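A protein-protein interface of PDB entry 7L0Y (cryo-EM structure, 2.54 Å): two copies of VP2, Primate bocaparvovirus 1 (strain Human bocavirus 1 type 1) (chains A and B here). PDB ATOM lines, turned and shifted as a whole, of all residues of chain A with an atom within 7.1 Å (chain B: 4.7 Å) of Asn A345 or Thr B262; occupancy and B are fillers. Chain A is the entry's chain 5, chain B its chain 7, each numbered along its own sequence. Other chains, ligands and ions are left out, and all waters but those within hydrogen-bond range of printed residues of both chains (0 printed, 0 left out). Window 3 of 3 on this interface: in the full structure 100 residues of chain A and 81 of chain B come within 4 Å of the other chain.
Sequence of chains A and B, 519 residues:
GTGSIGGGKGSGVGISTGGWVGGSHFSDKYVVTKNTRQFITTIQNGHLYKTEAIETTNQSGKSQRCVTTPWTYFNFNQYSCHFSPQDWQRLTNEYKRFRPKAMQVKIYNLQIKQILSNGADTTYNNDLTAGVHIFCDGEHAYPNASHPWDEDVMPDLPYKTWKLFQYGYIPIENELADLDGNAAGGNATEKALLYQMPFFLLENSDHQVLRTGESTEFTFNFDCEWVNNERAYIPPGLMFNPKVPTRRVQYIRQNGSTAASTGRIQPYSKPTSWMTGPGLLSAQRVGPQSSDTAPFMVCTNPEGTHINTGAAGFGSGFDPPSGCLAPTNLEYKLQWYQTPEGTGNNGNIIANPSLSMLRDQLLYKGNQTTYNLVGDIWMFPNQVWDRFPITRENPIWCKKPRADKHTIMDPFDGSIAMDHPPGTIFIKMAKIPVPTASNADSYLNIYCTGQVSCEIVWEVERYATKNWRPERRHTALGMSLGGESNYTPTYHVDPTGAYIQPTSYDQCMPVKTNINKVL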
ATOM      1  N   GLN A 289       1.917  13.614   6.886  1.00  0.00           N
ATOM      2  CA  GLN A 289       1.802  14.923   6.251  1.00  0.00           C
ATOM      3  C   GLN A 289       1.713  14.822   4.734  1.00  0.00           C
ATOM      4  O   GLN A 289       1.192  15.733   4.084  1.00  0.00           O
ATOM      5  CB  GLN A 289       3.004  15.794   6.615  1.00  0.00           C
ATOM      6  CG  GLN A 289       3.134  16.245   8.059  1.00  0.00           C
ATOM      7  CD  GLN A 289       2.058  17.217   8.481  1.00  0.00           C
ATOM      8  OE1 GLN A 289       1.245  16.924   9.348  1.00  0.00           O
ATOM      9  NE2 GLN A 289       2.017  18.361   7.825  1.00  0.00           N
ATOM     10  N   LEU A 330      -6.097  21.433  18.205  1.00  0.00           N
ATOM     11  CA  LEU A 330      -5.358  22.205  17.220  1.00  0.00           C
ATOM     12  C   LEU A 330      -5.701  21.809  15.791  1.00  0.00           C
ATOM     13  O   LEU A 330      -5.599  22.648  14.891  1.00  0.00           O
ATOM     14  CB  LEU A 330      -3.862  22.031  17.459  1.00  0.00           C
ATOM     15  CG  LEU A 330      -2.884  22.927  16.706  1.00  0.00           C
ATOM     16  CD1 LEU A 330      -3.457  24.317  16.574  1.00  0.00           C
ATOM     17  CD2 LEU A 330      -1.580  22.975  17.446  1.00  0.00           C
ATOM     18  N   GLN A 335      -5.174  27.390  10.138  1.00  0.00           N
ATOM     19  CA  GLN A 335      -3.761  27.647  10.336  1.00  0.00           C
ATOM     20  C   GLN A 335      -3.095  27.804   8.981  1.00  0.00           C
ATOM     21  O   GLN A 335      -3.426  27.097   8.030  1.00  0.00           O
ATOM     22  CB  GLN A 335      -3.124  26.515  11.142  1.00  0.00           C
ATOM     23  CG  GLN A 335      -1.752  26.799  11.671  1.00  0.00           C
ATOM     24  CD  GLN A 335      -1.283  25.709  12.593  1.00  0.00           C
ATOM     25  OE1 GLN A 335      -2.018  24.770  12.880  1.00  0.00           O
ATOM     26  NE2 GLN A 335      -0.060  25.827  13.071  1.00  0.00           N
ATOM     27  N   TYR A 337       0.696  29.671   6.870  1.00  0.00           N
ATOM     28  CA  TYR A 337       1.997  30.314   6.959  1.00  0.00           C
ATOM     29  C   TYR A 337       1.909  31.709   6.364  1.00  0.00           C
ATOM     30  O   TYR A 337       1.192  31.924   5.383  1.00  0.00           O
ATOM     31  CB  TYR A 337       3.086  29.517   6.240  1.00  0.00           C
ATOM     32  CG  TYR A 337       3.394  28.184   6.859  1.00  0.00           C
ATOM     33  CD1 TYR A 337       4.077  28.108   8.054  1.00  0.00           C
ATOM     34  CD2 TYR A 337       3.077  27.004   6.211  1.00  0.00           C
ATOM     35  CE1 TYR A 337       4.374  26.906   8.623  1.00  0.00           C
ATOM     36  CE2 TYR A 337       3.391  25.789   6.765  1.00  0.00           C
ATOM     37  CZ  TYR A 337       4.035  25.747   7.975  1.00  0.00           C
ATOM     38  OH  TYR A 337       4.347  24.543   8.547  1.00  0.00           O
ATOM     39  N   GLY A 342       7.747  29.359   4.995  1.00  0.00           N
ATOM     40  CA  GLY A 342       7.406  28.845   6.311  1.00  0.00           C
ATOM     41  C   GLY A 342       7.314  27.332   6.312  1.00  0.00           C
ATOM     42  O   GLY A 342       6.727  26.729   5.405  1.00  0.00           O
ATOM     43  N   THR A 343       7.892  26.708   7.336  1.00  0.00           N
ATOM     44  CA  THR A 343       7.869  25.264   7.511  1.00  0.00           C
ATOM     45  C   THR A 343       7.794  24.941   8.994  1.00  0.00           C
ATOM     46  O   THR A 343       8.355  25.652   9.829  1.00  0.00           O
ATOM     47  CB  THR A 343       9.112  24.576   6.916  1.00  0.00           C
ATOM     48  OG1 THR A 343      10.297  25.176   7.449  1.00  0.00           O
ATOM     49  CG2 THR A 343       9.132  24.662   5.404  1.00  0.00           C
ATOM     50  N   GLY A 344       7.103  23.853   9.313  1.00  0.00           N
ATOM     51  CA  GLY A 344       7.055  23.394  10.691  1.00  0.00           C
ATOM     52  C   GLY A 344       6.300  24.360  11.576  1.00  0.00           C
ATOM     53  O   GLY A 344       5.234  24.868  11.221  1.00  0.00           O
ATOM     54  N   ASN A 345       6.850  24.611  12.756  1.00  0.00           N
ATOM     55  CA  ASN A 345       6.288  25.562  13.701  1.00  0.00           C
ATOM     56  C   ASN A 345       6.813  26.970  13.490  1.00  0.00           C
ATOM     57  O   ASN A 345       6.520  27.855  14.297  1.00  0.00           O
ATOM     58  CB  ASN A 345       6.566  25.112  15.132  1.00  0.00           C
ATOM     59  CG  ASN A 345       5.699  23.955  15.552  1.00  0.00           C
ATOM     60  OD1 ASN A 345       4.587  23.801  15.069  1.00  0.00           O
ATOM     61  ND2 ASN A 345       6.211  23.124  16.450  1.00  0.00           N
ATOM     62  N   ASN A 346       7.595  27.189  12.446  1.00  0.00           N
ATOM     63  CA  ASN A 346       8.148  28.496  12.138  1.00  0.00           C
ATOM     64  C   ASN A 346       7.268  29.186  11.105  1.00  0.00           C
ATOM     65  O   ASN A 346       7.054  28.653  10.014  1.00  0.00           O
ATOM     66  CB  ASN A 346       9.577  28.370  11.613  1.00  0.00           C
ATOM     67  CG  ASN A 346      10.286  29.701  11.537  1.00  0.00           C
ATOM     68  OD1 ASN A 346      10.052  30.587  12.355  1.00  0.00           O
ATOM     69  ND2 ASN A 346      11.146  29.856  10.539  1.00  0.00           N
ATOM     70  N   GLY A 347       6.763  30.365  11.453  1.00  0.00           N
ATOM     71  CA  GLY A 347       6.035  31.178  10.505  1.00  0.00           C
ATOM     72  C   GLY A 347       4.566  30.865  10.371  1.00  0.00           C
ATOM     73  O   GLY A 347       3.928  31.344   9.434  1.00  0.00           O
ATOM     74  N   ASN A 348       4.005  30.085  11.287  1.00  0.00           N
ATOM     75  CA  ASN A 348       2.622  29.643  11.208  1.00  0.00           C
ATOM     76  C   ASN A 348       1.751  30.460  12.147  1.00  0.00           C
ATOM     77  O   ASN A 348       2.186  30.834  13.238  1.00  0.00           O
ATOM     78  CB  ASN A 348       2.511  28.158  11.541  1.00  0.00           C
ATOM     79  CG  ASN A 348       3.109  27.825  12.877  1.00  0.00           C
ATOM     80  OD1 ASN A 348       3.916  28.583  13.406  1.00  0.00           O
ATOM     81  ND2 ASN A 348       2.709  26.702  13.445  1.00  0.00           N
ATOM     82  N   ILE A 350      -1.990  30.406  13.996  1.00  0.00           N
ATOM     83  CA  ILE A 350      -3.138  29.618  14.404  1.00  0.00           C
ATOM     84  C   ILE A 350      -4.252  30.579  14.778  1.00  0.00           C
ATOM     85  O   ILE A 350      -4.039  31.509  15.561  1.00  0.00           O
ATOM     86  CB  ILE A 350      -2.780  28.716  15.591  1.00  0.00           C
ATOM     87  CG1 ILE A 350      -1.583  27.840  15.240  1.00  0.00           C
ATOM     88  CG2 ILE A 350      -3.958  27.861  15.957  1.00  0.00           C
ATOM     89  CD1 ILE A 350      -1.012  27.104  16.408  1.00  0.00           C
ATOM     90  N   VAL B 249      -1.988  25.290   6.672  1.00  0.00           N
ATOM     91  CA  VAL B 249      -1.206  24.387   7.504  1.00  0.00           C
ATOM     92  C   VAL B 249      -2.116  23.270   7.979  1.00  0.00           C
ATOM     93  O   VAL B 249      -3.266  23.518   8.356  1.00  0.00           O
ATOM     94  CB  VAL B 249      -0.587  25.120   8.707  1.00  0.00           C
ATOM     95  CG1 VAL B 249       0.103  24.147   9.625  1.00  0.00           C
ATOM     96  CG2 VAL B 249       0.376  26.151   8.250  1.00  0.00           C
ATOM     97  N   GLN B 250      -1.603  22.048   7.973  1.00  0.00           N
ATOM     98  CA  GLN B 250      -2.283  20.909   8.568  1.00  0.00           C
ATOM     99  C   GLN B 250      -1.489  20.425   9.774  1.00  0.00           C
ATOM    100  O   GLN B 250      -0.359  19.949   9.636  1.00  0.00           O
ATOM    101  CB  GLN B 250      -2.480  19.797   7.541  1.00  0.00           C
ATOM    102  CG  GLN B 250      -1.213  19.351   6.853  1.00  0.00           C
ATOM    103  CD  GLN B 250      -1.471  18.294   5.834  1.00  0.00           C
ATOM    104  OE1 GLN B 250      -2.596  18.128   5.373  1.00  0.00           O
ATOM    105  NE2 GLN B 250      -0.435  17.558   5.474  1.00  0.00           N
ATOM    106  N   TYR B 251      -2.070  20.580  10.953  1.00  0.00           N
ATOM    107  CA  TYR B 251      -1.534  20.008  12.175  1.00  0.00           C
ATOM    108  C   TYR B 251      -2.163  18.645  12.386  1.00  0.00           C
ATOM    109  O   TYR B 251      -3.387  18.513  12.337  1.00  0.00           O
ATOM    110  CB  TYR B 251      -1.821  20.900  13.380  1.00  0.00           C
ATOM    111  CG  TYR B 251      -1.438  20.269  14.689  1.00  0.00           C
ATOM    112  CD1 TYR B 251      -0.120  20.253  15.109  1.00  0.00           C
ATOM    113  CD2 TYR B 251      -2.391  19.674  15.499  1.00  0.00           C
ATOM    114  CE1 TYR B 251       0.234  19.677  16.300  1.00  0.00           C
ATOM    115  CE2 TYR B 251      -2.047  19.095  16.692  1.00  0.00           C
ATOM    116  CZ  TYR B 251      -0.733  19.100  17.090  1.00  0.00           C
ATOM    117  OH  TYR B 251      -0.377  18.525  18.284  1.00  0.00           O
ATOM    118  N   ALA B 260       3.147  14.276  17.036  1.00  0.00           N
ATOM    119  CA  ALA B 260       2.348  15.346  16.463  1.00  0.00           C
ATOM    120  C   ALA B 260       3.182  16.159  15.486  1.00  0.00           C
ATOM    121  O   ALA B 260       4.280  16.614  15.806  1.00  0.00           O
ATOM    122  CB  ALA B 260       1.795  16.245  17.564  1.00  0.00           C
ATOM    123  N   SER B 261       2.654  16.337  14.283  1.00  0.00           N
ATOM    124  CA  SER B 261       3.367  17.033  13.228  1.00  0.00           C
ATOM    125  C   SER B 261       2.523  18.182  12.707  1.00  0.00           C
ATOM    126  O   SER B 261       1.292  18.139  12.739  1.00  0.00           O
ATOM    127  CB  SER B 261       3.727  16.088  12.076  1.00  0.00           C
ATOM    128  OG  SER B 261       2.564  15.561  11.466  1.00  0.00           O
ATOM    129  N   THR B 262       3.206  19.215  12.238  1.00  0.00           N
ATOM    130  CA  THR B 262       2.586  20.329  11.545  1.00  0.00           C
ATOM    131  C   THR B 262       3.368  20.571  10.265  1.00  0.00           C
ATOM    132  O   THR B 262       4.569  20.296  10.206  1.00  0.00           O
ATOM    133  CB  THR B 262       2.561  21.585  12.415  1.00  0.00           C
ATOM    134  OG1 THR B 262       1.791  22.600  11.771  1.00  0.00           O
ATOM    135  CG2 THR B 262       3.956  22.104  12.627  1.00  0.00           C
ATOM    136  N   GLY B 263       2.687  21.051   9.238  1.00  0.00           N
ATOM    137  CA  GLY B 263       3.342  21.278   7.970  1.00  0.00           C
ATOM    138  C   GLY B 263       2.382  21.876   6.972  1.00  0.00           C
ATOM    139  O   GLY B 263       1.187  22.029   7.234  1.00  0.00           O
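No position is printed for both chains. Of the 12 pairs that touch across the chains among the printed residues, none has its exchanged pair printed and touching as well.
ND2 of Asn A348 lies close to NE2 of Gln A335 (2.9 Å). The side-chain hydroxyl of Tyr A337 sits at hydrogen-bond distance from the backbone carbonyl oxygen of Gly A344 (2.8 Å). The backbone carbonyl oxygen (O) of Asn A345 sits close to the side-chain amide oxygen (OD1) of Asn A348 (2.8 Å). N of Gln B250 sits at hydrogen-bond distance from O of Gly B263 (2.9 Å).
Of the printed residues of chain A, Thr B262 touches Gln A289, Gln A335, Gly A344 and Asn A345. Printed residues of chain A within 4 Å of Gly B263: Gln A289 and Tyr A337. Printed residues of chain B within 4 Å of Gln A289: Gln B250, Ser B261, Thr B262 and Gly B263. Printed residues of chain A within 4 Å of Tyr B251: Leu A330 (3.4 Å) and Gln A335 (3.9 Å). Of the printed residues of chain A, Ser B261 touches Gln A289 (2.8 Å). Of the printed residues of chain B, Gly A344 touches Thr B262. The nearest printed residue of chain B that does not touch Asn A345 is Tyr B251 (5.9 Å). The nearest residue of chain A that does not touch Thr B262 is Tyr A337 (4.4 Å). The nearest printed residue of chain A that does not touch Gly B263 is Gly A344 (4.8 Å).
NE2 of Gln A289 touches C of Thr B262, 3.6 Å away. Leu A330 touches Tyr B251. Tyr B251 touches Gln A335. NE2 of Gln A335 touches OG1 of Thr B262, 3.9 Å away. CE2 of Tyr A337 touches CG2 of Val B249 (3.4 Å). Gly B263 touches Tyr A337 (CA to OH, 3.5 Å). O of Gly A344 touches CG2 of Thr B262, 3.4 Å away. Asn A345 touches Thr B262 (OD1 to CG2, 3.0 Å).
The backbone carbonyl oxygen of Gln A289 sits at hydrogen-bond distance from the side-chain amide nitrogen of Gln B250. OE1 of Gln A289 lies within hydrogen-bond range of OG of Ser B261 (2.8 Å). N of Gly B263 lies close to NE2 of Gln A289 (3.1 Å). O of Gln A335 is in hydrogen-bond range of N of Val B249, at 2.7 Å.
Of the 12 printed residues of chain A, 6 touch a printed residue of chain B. Hydrophobic or aromatic side chains of chain A that line the printed part of chain B: Leu A330 and Tyr A337. Among the printed residues, 12 pairs touch across the chains. Among the printed residues, no Asp or Glu carboxylate lies within 4 Å of a Lys or Arg side-chain nitrogen of the other chain.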
